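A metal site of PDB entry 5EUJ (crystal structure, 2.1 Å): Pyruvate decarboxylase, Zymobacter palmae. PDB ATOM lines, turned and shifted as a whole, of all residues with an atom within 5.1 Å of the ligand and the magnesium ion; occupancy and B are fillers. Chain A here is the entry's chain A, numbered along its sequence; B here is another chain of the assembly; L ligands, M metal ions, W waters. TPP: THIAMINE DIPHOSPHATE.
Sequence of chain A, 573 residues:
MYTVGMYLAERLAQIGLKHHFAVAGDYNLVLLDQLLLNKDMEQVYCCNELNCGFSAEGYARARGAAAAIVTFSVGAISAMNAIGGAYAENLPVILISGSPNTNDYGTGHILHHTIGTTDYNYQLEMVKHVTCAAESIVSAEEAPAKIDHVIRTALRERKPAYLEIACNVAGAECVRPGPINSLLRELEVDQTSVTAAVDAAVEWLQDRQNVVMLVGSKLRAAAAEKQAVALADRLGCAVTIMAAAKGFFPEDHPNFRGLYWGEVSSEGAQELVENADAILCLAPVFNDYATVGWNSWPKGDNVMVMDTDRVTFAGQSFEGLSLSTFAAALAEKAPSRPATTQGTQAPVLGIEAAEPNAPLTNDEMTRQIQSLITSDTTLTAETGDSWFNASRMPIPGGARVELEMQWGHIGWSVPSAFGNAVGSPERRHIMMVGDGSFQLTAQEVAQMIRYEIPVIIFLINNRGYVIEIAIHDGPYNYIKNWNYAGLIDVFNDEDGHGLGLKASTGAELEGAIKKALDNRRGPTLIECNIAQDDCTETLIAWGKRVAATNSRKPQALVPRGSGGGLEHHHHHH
The backbone NH of Asp 385 is in hydrogen-bond range of an oxygen (O2B) of the ligand.
N of Gly 436 lies close to O2A of the ligand, 2.9 Å away.
The backbone carbonyl oxygen (O) of Gly 408 is in hydrogen-bond range of a nitrogen (N4') of the ligand (2.6 Å).
N of Asp 435 sits close to O2A of the ligand (3.5 Å).
An oxygen (O1A) of the ligand is in hydrogen-bond range of the backbone NH (N) of Ser 437 (2.7 Å).
An oxygen (O1B) of the ligand is in hydrogen-bond range of the backbone NH (N) of Val 466 (3.3 Å).
The side-chain carboxylate (OE2) of Glu 49 of chain B lies within hydrogen-bond range of a nitrogen (N1') of the ligand.
OG of Ser 437 lies within hydrogen-bond range of O1A of the ligand.
N of Ile 467 sits at hydrogen-bond distance from O1B of the ligand, 2.8 Å away.
N of Ile 410 lies within hydrogen-bond range of N3' of the ligand.
OD2 of Asp 435 is in hydrogen-bond range of N of Arg 463, at 3.2 Å.
O of Ile 460 sits at hydrogen-bond distance from N of Asp 435, at 3.1 Å.
The backbone NH of Asp 26 of chain B lies within hydrogen-bond range of the side-chain carboxylate of Glu 468, at 3.2 Å.
OG of Ser 437 sits at hydrogen-bond distance from O of Thr 383 (3.4 Å).
Thr 383 touches the ligand.
Gly 384 touches the ligand.
His 409 touches the ligand.
CA of Gly 434 touches O1A of the ligand (3.4 Å).
Leu 440 touches the ligand (CD2 to CM2, 3.8 Å).
Tyr 465 touches the ligand.
Glu 468 touches the ligand.
Ala 24 of chain B touches the ligand (O to C6', 3.3 Å).
Gly 25 of chain B touches the ligand.
Val 74 of chain B touches the ligand (CG2 to N3', 3.5 Å).
His 113 of chain B touches the ligand.
Hydrophobic or aromatic side chains within 4 Å of the ligand: His 409, Ile 410, Leu 440, Tyr 465, Val 466, Ile 467, Val 74 of chain B and His 113 of chain B.
The nearest printed residue that does not touch the ligand is Thr 71 of chain B (4.1 Å).
Within 4 Å of the magnesium ion: Asp 435, Asn 462 and Gly 464.
The nearest printed residue that does not touch the magnesium ion is Gly 436 (4.1 Å).
O2A of the ligand binds the magnesium ion, 1.9 Å away.
The magnesium ion is bound by O3B of the ligand, 2.1 Å away.
The side-chain carboxylate (OD1) of Asp 435 is bound to the magnesium ion, at 2.1 Å.
The magnesium ion is bound by the backbone carbonyl oxygen (O) of Gly 464, at 2.1 Å.
OD1 of Asn 462 binds the magnesium ion (2.2 Å).
Water W4 is bound to the magnesium ion, at 2.2 Å.
Water W4 lies within hydrogen-bond range of O of Ile 460 (2.8 Å), O2B of the ligand (3.1 Å), ND2 of Asn 462 (3.2 Å) and N of Asp 435 (3.3 Å).
Water W2 lies within hydrogen-bond range of the backbone carbonyl oxygen of Thr 383 (2.7 Å), the backbone NH of Gly 434 (2.9 Å), an oxygen (O1A) of the ligand (2.9 Å) and the side-chain hydroxyl of Ser 437 (3.1 Å).
Water W3 bridges OG of Ser 386 (2.6 Å) and O2B of the ligand (3.0 Å).
Water W1 bridges the side-chain carboxylate (OE2) of Glu 468 (2.7 Å) and the side-chain carboxylate (OD1) of Asp 26 of chain B (3.3 Å).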
ATOM      1  N   GLU A 382     -23.314  25.055 -17.792  1.00  0.00           N
ATOM      2  CA  GLU A 382     -22.190  24.429 -17.093  1.00  0.00           C
ATOM      3  C   GLU A 382     -22.071  22.947 -17.384  1.00  0.00           C
ATOM      4  O   GLU A 382     -23.071  22.278 -17.667  1.00  0.00           O
ATOM      5  CB  GLU A 382     -22.379  24.665 -15.595  1.00  0.00           C
ATOM      6  CG  GLU A 382     -21.266  24.169 -14.673  1.00  0.00           C
ATOM      7  CD  GLU A 382     -19.902  24.722 -14.996  1.00  0.00           C
ATOM      8  OE1 GLU A 382     -19.249  24.156 -15.885  1.00  0.00           O
ATOM      9  OE2 GLU A 382     -19.480  25.716 -14.355  1.00  0.00           O
ATOM     10  N   THR A 383     -20.843  22.426 -17.317  1.00  0.00           N
ATOM     11  CA  THR A 383     -20.585  20.974 -17.264  1.00  0.00           C
ATOM     12  C   THR A 383     -21.399  20.347 -16.118  1.00  0.00           C
ATOM     13  O   THR A 383     -21.383  20.839 -15.002  1.00  0.00           O
ATOM     14  CB  THR A 383     -19.084  20.685 -17.058  1.00  0.00           C
ATOM     15  OG1 THR A 383     -18.325  21.234 -18.152  1.00  0.00           O
ATOM     16  CG2 THR A 383     -18.813  19.192 -16.977  1.00  0.00           C
ATOM     17  N   GLY A 384     -22.111  19.266 -16.423  1.00  0.00           N
ATOM     18  CA  GLY A 384     -23.126  18.715 -15.526  1.00  0.00           C
ATOM     19  C   GLY A 384     -24.332  18.287 -16.335  1.00  0.00           C
ATOM     20  O   GLY A 384     -24.262  18.225 -17.568  1.00  0.00           O
ATOM     21  N   ASP A 385     -25.447  18.019 -15.669  1.00  0.00           N
ATOM     22  CA  ASP A 385     -26.699  17.685 -16.369  1.00  0.00           C
ATOM     23  C   ASP A 385     -27.235  18.860 -17.205  1.00  0.00           C
ATOM     24  O   ASP A 385     -28.034  18.642 -18.111  1.00  0.00           O
ATOM     25  CB  ASP A 385     -27.775  17.218 -15.375  1.00  0.00           C
ATOM     26  CG  ASP A 385     -28.906  16.441 -16.048  1.00  0.00           C
ATOM     27  OD1 ASP A 385     -28.677  15.732 -17.051  1.00  0.00           O
ATOM     28  OD2 ASP A 385     -30.045  16.519 -15.556  1.00  0.00           O
ATOM     29  N   SER A 386     -26.790  20.087 -16.886  1.00  0.00           N
ATOM     30  CA  SER A 386     -27.025  21.270 -17.720  1.00  0.00           C
ATOM     31  C   SER A 386     -26.602  21.136 -19.189  1.00  0.00           C
ATOM     32  O   SER A 386     -27.195  21.785 -20.056  1.00  0.00           O
ATOM     33  CB  SER A 386     -26.319  22.476 -17.110  1.00  0.00           C
ATOM     34  OG  SER A 386     -26.948  22.907 -15.919  1.00  0.00           O
ATOM     35  N   GLY A 408     -14.124  21.423 -20.048  1.00  0.00           N
ATOM     36  CA  GLY A 408     -15.041  20.846 -19.074  1.00  0.00           C
ATOM     37  C   GLY A 408     -14.686  21.075 -17.617  1.00  0.00           C
ATOM     38  O   GLY A 408     -14.823  20.172 -16.802  1.00  0.00           O
ATOM     39  N   HIS A 409     -14.227  22.276 -17.298  1.00  0.00           N
ATOM     40  CA  HIS A 409     -13.825  22.649 -15.946  1.00  0.00           C
ATOM     41  C   HIS A 409     -15.058  23.121 -15.178  1.00  0.00           C
ATOM     42  O   HIS A 409     -15.601  24.181 -15.478  1.00  0.00           O
ATOM     43  CB  HIS A 409     -12.795  23.755 -16.024  1.00  0.00           C
ATOM     44  CG  HIS A 409     -12.219  24.172 -14.701  1.00  0.00           C
ATOM     45  ND1 HIS A 409     -12.967  24.761 -13.704  1.00  0.00           N
ATOM     46  CD2 HIS A 409     -10.946  24.132 -14.248  1.00  0.00           C
ATOM     47  CE1 HIS A 409     -12.173  25.039 -12.681  1.00  0.00           C
ATOM     48  NE2 HIS A 409     -10.944  24.672 -12.984  1.00  0.00           N
ATOM     49  N   ILE A 410     -15.494  22.356 -14.190  1.00  0.00           N
ATOM     50  CA  ILE A 410     -16.696  22.750 -13.434  1.00  0.00           C
ATOM     51  C   ILE A 410     -16.415  24.033 -12.671  1.00  0.00           C
ATOM     52  O   ILE A 410     -15.306  24.247 -12.192  1.00  0.00           O
ATOM     53  CB  ILE A 410     -17.261  21.645 -12.519  1.00  0.00           C
ATOM     54  CG1 ILE A 410     -16.228  21.108 -11.514  1.00  0.00           C
ATOM     55  CG2 ILE A 410     -17.830  20.521 -13.377  1.00  0.00           C
ATOM     56  CD1 ILE A 410     -16.871  20.456 -10.321  1.00  0.00           C
ATOM     57  N   GLY A 434     -24.758  23.824 -11.849  1.00  0.00           N
ATOM     58  CA  GLY A 434     -25.062  22.855 -10.800  1.00  0.00           C
ATOM     59  C   GLY A 434     -24.519  23.319  -9.464  1.00  0.00           C
ATOM     60  O   GLY A 434     -23.730  24.258  -9.393  1.00  0.00           O
ATOM     61  N   ASP A 435     -24.956  22.644  -8.411  1.00  0.00           N
ATOM     62  CA  ASP A 435     -24.509  22.970  -7.057  1.00  0.00           C
ATOM     63  C   ASP A 435     -23.000  22.696  -6.869  1.00  0.00           C
ATOM     64  O   ASP A 435     -22.295  23.518  -6.292  1.00  0.00           O
ATOM     65  CB  ASP A 435     -25.375  22.269  -5.987  1.00  0.00           C
ATOM     66  CG  ASP A 435     -25.423  20.745  -6.132  1.00  0.00           C
ATOM     67  OD1 ASP A 435     -25.429  20.205  -7.256  1.00  0.00           O
ATOM     68  OD2 ASP A 435     -25.493  20.064  -5.088  1.00  0.00           O
ATOM     69  N   GLY A 436     -22.522  21.581  -7.393  1.00  0.00           N
ATOM     70  CA  GLY A 436     -21.111  21.222  -7.296  1.00  0.00           C
ATOM     71  C   GLY A 436     -20.205  22.233  -7.980  1.00  0.00           C
ATOM     72  O   GLY A 436     -19.279  22.774  -7.371  1.00  0.00           O
ATOM     73  N   SER A 437     -20.505  22.489  -9.256  1.00  0.00           N
ATOM     74  CA  SER A 437     -19.797  23.500 -10.043  1.00  0.00           C
ATOM     75  C   SER A 437     -19.749  24.833  -9.356  1.00  0.00           C
ATOM     76  O   SER A 437     -18.693  25.457  -9.239  1.00  0.00           O
ATOM     77  CB  SER A 437     -20.468  23.668 -11.396  1.00  0.00           C
ATOM     78  OG  SER A 437     -20.378  22.478 -12.157  1.00  0.00           O
ATOM     79  N   PHE A 438     -20.917  25.279  -8.897  1.00  0.00           N
ATOM     80  CA  PHE A 438     -21.060  26.587  -8.268  1.00  0.00           C
ATOM     81  C   PHE A 438     -20.088  26.794  -7.104  1.00  0.00           C
ATOM     82  O   PHE A 438     -19.541  27.889  -6.939  1.00  0.00           O
ATOM     83  CB  PHE A 438     -22.499  26.801  -7.801  1.00  0.00           C
ATOM     84  CG  PHE A 438     -22.774  28.211  -7.346  1.00  0.00           C
ATOM     85  CD1 PHE A 438     -23.010  29.221  -8.282  1.00  0.00           C
ATOM     86  CD2 PHE A 438     -22.785  28.525  -6.003  1.00  0.00           C
ATOM     87  CE1 PHE A 438     -23.249  30.523  -7.869  1.00  0.00           C
ATOM     88  CE2 PHE A 438     -23.021  29.818  -5.580  1.00  0.00           C
ATOM     89  CZ  PHE A 438     -23.251  30.828  -6.508  1.00  0.00           C
ATOM     90  N   LEU A 440     -17.033  25.738  -6.680  1.00  0.00           N
ATOM     91  CA  LEU A 440     -15.658  26.064  -7.089  1.00  0.00           C
ATOM     92  C   LEU A 440     -15.409  27.554  -7.280  1.00  0.00           C
ATOM     93  O   LEU A 440     -14.308  28.030  -6.987  1.00  0.00           O
ATOM     94  CB  LEU A 440     -15.252  25.339  -8.384  1.00  0.00           C
ATOM     95  CG  LEU A 440     -14.819  23.882  -8.235  1.00  0.00           C
ATOM     96  CD1 LEU A 440     -15.995  22.944  -8.394  1.00  0.00           C
ATOM     97  CD2 LEU A 440     -13.714  23.543  -9.229  1.00  0.00           C
ATOM     98  N   ILE A 460     -28.975  24.542 -10.059  1.00  0.00           N
ATOM     99  CA  ILE A 460     -29.639  23.240  -9.882  1.00  0.00           C
ATOM    100  C   ILE A 460     -29.094  22.613  -8.607  1.00  0.00           C
ATOM    101  O   ILE A 460     -27.972  22.084  -8.587  1.00  0.00           O
ATOM    102  CB  ILE A 460     -29.411  22.274 -11.075  1.00  0.00           C
ATOM    103  CG1 ILE A 460     -30.083  22.804 -12.346  1.00  0.00           C
ATOM    104  CG2 ILE A 460     -29.950  20.876 -10.757  1.00  0.00           C
ATOM    105  CD1 ILE A 460     -29.225  23.737 -13.169  1.00  0.00           C
ATOM    106  N   ASN A 462     -29.257  19.674  -6.721  1.00  0.00           N
ATOM    107  CA  ASN A 462     -29.595  18.259  -6.663  1.00  0.00           C
ATOM    108  C   ASN A 462     -28.720  17.468  -5.683  1.00  0.00           C
ATOM    109  O   ASN A 462     -28.656  16.246  -5.755  1.00  0.00           O
ATOM    110  CB  ASN A 462     -29.578  17.636  -8.079  1.00  0.00           C
ATOM    111  CG  ASN A 462     -28.236  17.790  -8.777  1.00  0.00           C
ATOM    112  OD1 ASN A 462     -27.236  18.196  -8.176  1.00  0.00           O
ATOM    113  ND2 ASN A 462     -28.207  17.469 -10.072  1.00  0.00           N
ATOM    114  N   ARG A 463     -28.041  18.177  -4.778  1.00  0.00           N
ATOM    115  CA  ARG A 463     -27.331  17.559  -3.648  1.00  0.00           C
ATOM    116  C   ARG A 463     -26.235  16.594  -4.127  1.00  0.00           C
ATOM    117  O   ARG A 463     -26.192  15.418  -3.736  1.00  0.00           O
ATOM    118  CB  ARG A 463     -28.331  16.850  -2.715  1.00  0.00           C
ATOM    119  CG  ARG A 463     -29.491  17.730  -2.229  1.00  0.00           C
ATOM    120  CD  ARG A 463     -28.998  18.920  -1.425  1.00  0.00           C
ATOM    121  NE  ARG A 463     -28.072  18.481  -0.377  1.00  0.00           N
ATOM    122  CZ  ARG A 463     -28.427  18.007   0.831  1.00  0.00           C
ATOM    123  NH1 ARG A 463     -29.708  17.936   1.214  1.00  0.00           N
ATOM    124  NH2 ARG A 463     -27.471  17.623   1.684  1.00  0.00           N
ATOM    125  N   GLY A 464     -25.368  17.078  -5.017  1.00  0.00           N
ATOM    126  CA  GLY A 464     -24.229  16.297  -5.473  1.00  0.00           C
ATOM    127  C   GLY A 464     -23.814  16.440  -6.919  1.00  0.00           C
ATOM    128  O   GLY A 464     -24.406  17.191  -7.709  1.00  0.00           O
ATOM    129  N   TYR A 465     -22.763  15.696  -7.247  1.00  0.00           N
ATOM    130  CA  TYR A 465     -22.189  15.642  -8.566  1.00  0.00           C
ATOM    131  C   TYR A 465     -22.930  14.558  -9.358  1.00  0.00           C
ATOM    132  O   TYR A 465     -22.458  13.430  -9.468  1.00  0.00           O
ATOM    133  CB  TYR A 465     -20.700  15.250  -8.452  1.00  0.00           C
ATOM    134  CG  TYR A 465     -19.750  16.203  -7.742  1.00  0.00           C
ATOM    135  CD1 TYR A 465     -19.939  17.586  -7.711  1.00  0.00           C
ATOM    136  CD2 TYR A 465     -18.575  15.709  -7.151  1.00  0.00           C
ATOM    137  CE1 TYR A 465     -19.017  18.431  -7.093  1.00  0.00           C
ATOM    138  CE2 TYR A 465     -17.657  16.532  -6.543  1.00  0.00           C
ATOM    139  CZ  TYR A 465     -17.869  17.891  -6.509  1.00  0.00           C
ATOM    140  OH  TYR A 465     -16.931  18.688  -5.891  1.00  0.00           O
ATOM    141  N   VAL A 466     -24.095  14.906  -9.909  1.00  0.00           N
ATOM    142  CA  VAL A 466     -25.005  13.896 -10.527  1.00  0.00           C
ATOM    143  C   VAL A 466     -24.445  13.236 -11.784  1.00  0.00           C
ATOM    144  O   VAL A 466     -24.632  12.048 -11.981  1.00  0.00           O
ATOM    145  CB  VAL A 466     -26.431  14.478 -10.757  1.00  0.00           C
ATOM    146  CG1 VAL A 466     -27.289  13.592 -11.658  1.00  0.00           C
ATOM    147  CG2 VAL A 466     -27.115  14.640  -9.405  1.00  0.00           C
ATOM    148  N   ILE A 467     -23.795  14.005 -12.632  1.00  0.00           N
ATOM    149  CA  ILE A 467     -23.107  13.450 -13.808  1.00  0.00           C
ATOM    150  C   ILE A 467     -21.988  12.441 -13.435  1.00  0.00           C
ATOM    151  O   ILE A 467     -21.800  11.447 -14.140  1.00  0.00           O
ATOM    152  CB  ILE A 467     -22.572  14.572 -14.738  1.00  0.00           C
ATOM    153  CG1 ILE A 467     -21.878  14.022 -15.980  1.00  0.00           C
ATOM    154  CG2 ILE A 467     -21.586  15.454 -14.006  1.00  0.00           C
ATOM    155  CD1 ILE A 467     -21.818  15.018 -17.122  1.00  0.00           C
ATOM    156  N   GLU A 468     -21.270  12.706 -12.344  1.00  0.00           N
ATOM    157  CA  GLU A 468     -20.284  11.740 -11.835  1.00  0.00           C
ATOM    158  C   GLU A 468     -20.938  10.490 -11.267  1.00  0.00           C
ATOM    159  O   GLU A 468     -20.405   9.398 -11.408  1.00  0.00           O
ATOM    160  CB  GLU A 468     -19.370  12.354 -10.769  1.00  0.00           C
ATOM    161  CG  GLU A 468     -18.445  13.441 -11.279  1.00  0.00           C
ATOM    162  CD  GLU A 468     -17.390  12.917 -12.253  1.00  0.00           C
ATOM    163  OE1 GLU A 468     -16.418  12.277 -11.801  1.00  0.00           O
ATOM    164  OE2 GLU A 468     -17.554  13.142 -13.468  1.00  0.00           O
ATOM    165  N   VAL B  23     -10.460  15.824  -4.976  1.00  0.00           N
ATOM    166  CA  VAL B  23     -11.610  16.313  -5.746  1.00  0.00           C
ATOM    167  C   VAL B  23     -11.847  15.292  -6.859  1.00  0.00           C
ATOM    168  O   VAL B  23     -10.969  15.035  -7.671  1.00  0.00           O
ATOM    169  CB  VAL B  23     -11.349  17.708  -6.344  1.00  0.00           C
ATOM    170  CG1 VAL B  23     -12.589  18.208  -7.098  1.00  0.00           C
ATOM    171  CG2 VAL B  23     -10.974  18.680  -5.247  1.00  0.00           C
ATOM    172  N   ALA B  24     -13.032  14.699  -6.881  1.00  0.00           N
ATOM    173  CA  ALA B  24     -13.332  13.638  -7.836  1.00  0.00           C
ATOM    174  C   ALA B  24     -13.377  14.161  -9.270  1.00  0.00           C
ATOM    175  O   ALA B  24     -13.625  15.336  -9.486  1.00  0.00           O
ATOM    176  CB  ALA B  24     -14.647  12.952  -7.502  1.00  0.00           C
ATOM    177  N   GLY B  25     -13.106  13.249 -10.208  1.00  0.00           N
ATOM    178  CA  GLY B  25     -13.298  13.480 -11.627  1.00  0.00           C
ATOM    179  C   GLY B  25     -13.158  12.130 -12.304  1.00  0.00           C
ATOM    180  O   GLY B  25     -12.505  11.249 -11.759  1.00  0.00           O
ATOM    181  N   ASP B  26     -13.753  11.958 -13.471  1.00  0.00           N
ATOM    182  CA  ASP B  26     -13.829  10.613 -14.063  1.00  0.00           C
ATOM    183  C   ASP B  26     -12.468   9.911 -14.273  1.00  0.00           C
ATOM    184  O   ASP B  26     -12.407   8.692 -14.242  1.00  0.00           O
ATOM    185  CB  ASP B  26     -14.744  10.553 -15.303  1.00  0.00           C
ATOM    186  CG  ASP B  26     -14.221  11.346 -16.517  1.00  0.00           C
ATOM    187  OD1 ASP B  26     -13.310  12.207 -16.375  1.00  0.00           O
ATOM    188  OD2 ASP B  26     -14.770  11.088 -17.621  1.00  0.00           O
ATOM    189  N   GLU B  49      -9.658  22.463  -6.512  1.00  0.00           N
ATOM    190  CA  GLU B  49      -8.355  21.810  -6.490  1.00  0.00           C
ATOM    191  C   GLU B  49      -7.257  22.716  -5.964  1.00  0.00           C
ATOM    192  O   GLU B  49      -6.304  22.213  -5.360  1.00  0.00           O
ATOM    193  CB  GLU B  49      -8.000  21.263  -7.881  1.00  0.00           C
ATOM    194  CG  GLU B  49      -8.900  20.116  -8.322  1.00  0.00           C
ATOM    195  CD  GLU B  49     -10.153  20.567  -9.079  1.00  0.00           C
ATOM    196  OE1 GLU B  49     -10.499  21.762  -9.061  1.00  0.00           O
ATOM    197  OE2 GLU B  49     -10.782  19.699  -9.702  1.00  0.00           O
ATOM    198  N   THR B  71      -8.097  15.362 -10.773  1.00  0.00           N
ATOM    199  CA  THR B  71      -8.340  14.841 -12.119  1.00  0.00           C
ATOM    200  C   THR B  71      -7.448  15.571 -13.121  1.00  0.00           C
ATOM    201  O   THR B  71      -6.886  16.626 -12.819  1.00  0.00           O
ATOM    202  CB  THR B  71      -9.836  14.926 -12.507  1.00  0.00           C
ATOM    203  OG1 THR B  71     -10.096  14.065 -13.612  1.00  0.00           O
ATOM    204  CG2 THR B  71     -10.269  16.343 -12.880  1.00  0.00           C
ATOM    205  N   VAL B  74      -7.908  19.884 -15.750  1.00  0.00           N
ATOM    206  CA  VAL B  74      -8.854  20.803 -15.110  1.00  0.00           C
ATOM    207  C   VAL B  74      -8.612  20.875 -13.610  1.00  0.00           C
ATOM    208  O   VAL B  74      -8.693  21.960 -13.020  1.00  0.00           O
ATOM    209  CB  VAL B  74     -10.331  20.477 -15.433  1.00  0.00           C
ATOM    210  CG1 VAL B  74     -10.625  20.834 -16.874  1.00  0.00           C
ATOM    211  CG2 VAL B  74     -10.690  19.033 -15.148  1.00  0.00           C
ATOM    212  N   GLY B  75      -8.248  19.740 -12.995  1.00  0.00           N
ATOM    213  CA  GLY B  75      -7.871  19.723 -11.596  1.00  0.00           C
ATOM    214  C   GLY B  75      -6.422  20.090 -11.376  1.00  0.00           C
ATOM    215  O   GLY B  75      -6.099  21.068 -10.712  1.00  0.00           O
ATOM    216  N   HIS B 113     -11.043  17.264 -21.084  1.00  0.00           N
ATOM    217  CA  HIS B 113     -10.107  17.934 -20.169  1.00  0.00           C
ATOM    218  C   HIS B 113      -8.692  18.074 -20.724  1.00  0.00           C
ATOM    219  O   HIS B 113      -7.763  18.111 -19.954  1.00  0.00           O
ATOM    220  CB  HIS B 113      -9.989  17.225 -18.781  1.00  0.00           C
ATOM    221  CG  HIS B 113     -11.292  16.993 -18.087  1.00  0.00           C
ATOM    222  ND1 HIS B 113     -12.378  17.844 -18.202  1.00  0.00           N
ATOM    223  CD2 HIS B 113     -11.674  16.036 -17.204  1.00  0.00           C
ATOM    224  CE1 HIS B 113     -13.363  17.399 -17.461  1.00  0.00           C
ATOM    225  NE2 HIS B 113     -12.958  16.306 -16.837  1.00  0.00           N
HETATM  226  N1' TPP L   1     -12.956  19.289 -11.190  1.00  0.00           N
HETATM  227  C2' TPP L   1     -12.922  20.191 -12.215  1.00  0.00           C
HETATM  228  CM2 TPP L   1     -12.206  21.491 -12.033  1.00  0.00           C
HETATM  229  N3' TPP L   1     -13.553  19.945 -13.382  1.00  0.00           N
HETATM  230  C4' TPP L   1     -14.216  18.778 -13.564  1.00  0.00           C
HETATM  231  N4' TPP L   1     -14.806  18.558 -14.748  1.00  0.00           N
HETATM  232  C5' TPP L   1     -14.241  17.773 -12.460  1.00  0.00           C
HETATM  233  C6' TPP L   1     -13.579  18.106 -11.290  1.00  0.00           C
HETATM  234  C7' TPP L   1     -14.980  16.446 -12.601  1.00  0.00           C
HETATM  235  N3  TPP L   1     -16.450  16.629 -12.658  1.00  0.00           N
HETATM  236  C2  TPP L   1     -17.140  16.694 -13.825  1.00  0.00           C
HETATM  237  S1  TPP L   1     -18.880  16.932 -13.794  1.00  0.00           S
HETATM  238  C5  TPP L   1     -18.701  16.936 -12.063  1.00  0.00           C
HETATM  239  C4  TPP L   1     -17.294  16.746 -11.600  1.00  0.00           C
HETATM  240  CM4 TPP L   1     -16.935  16.706 -10.138  1.00  0.00           C
HETATM  241  C6  TPP L   1     -19.984  17.101 -11.301  1.00  0.00           C
HETATM  242  C7  TPP L   1     -20.690  18.431 -11.550  1.00  0.00           C
HETATM  243  O7  TPP L   1     -21.661  18.564 -10.510  1.00  0.00           O
HETATM  244  PA  TPP L   1     -22.803  19.673 -10.565  1.00  0.00           P
HETATM  245  O1A TPP L   1     -22.188  21.001 -10.842  1.00  0.00           O
HETATM  246  O2A TPP L   1     -23.568  19.588  -9.284  1.00  0.00           O
HETATM  247  O3A TPP L   1     -23.640  19.139 -11.835  1.00  0.00           O
HETATM  248  PB  TPP L   1     -24.760  17.981 -11.879  1.00  0.00           P
HETATM  249  O1B TPP L   1     -24.162  16.814 -12.604  1.00  0.00           O
HETATM  250  O2B TPP L   1     -25.904  18.654 -12.637  1.00  0.00           O
HETATM  251  O3B TPP L   1     -25.138  17.637 -10.465  1.00  0.00           O
HETATM  252 MG    MG M   1     -25.238  18.784  -8.753  1.00  0.00          MG
HETATM  253  O   HOH W   1     -15.719  14.167 -15.221  1.00  0.00           O
HETATM  254  O   HOH W   2     -23.212  21.943 -13.348  1.00  0.00           O
HETATM  255  O   HOH W   3     -25.923  21.267 -14.172  1.00  0.00           O
HETATM  256  O   HOH W   4     -26.452  20.182  -9.980  1.00  0.00           O
HETATM  257  O   HOH W   5     -17.605  15.511 -16.773  1.00  0.00           O
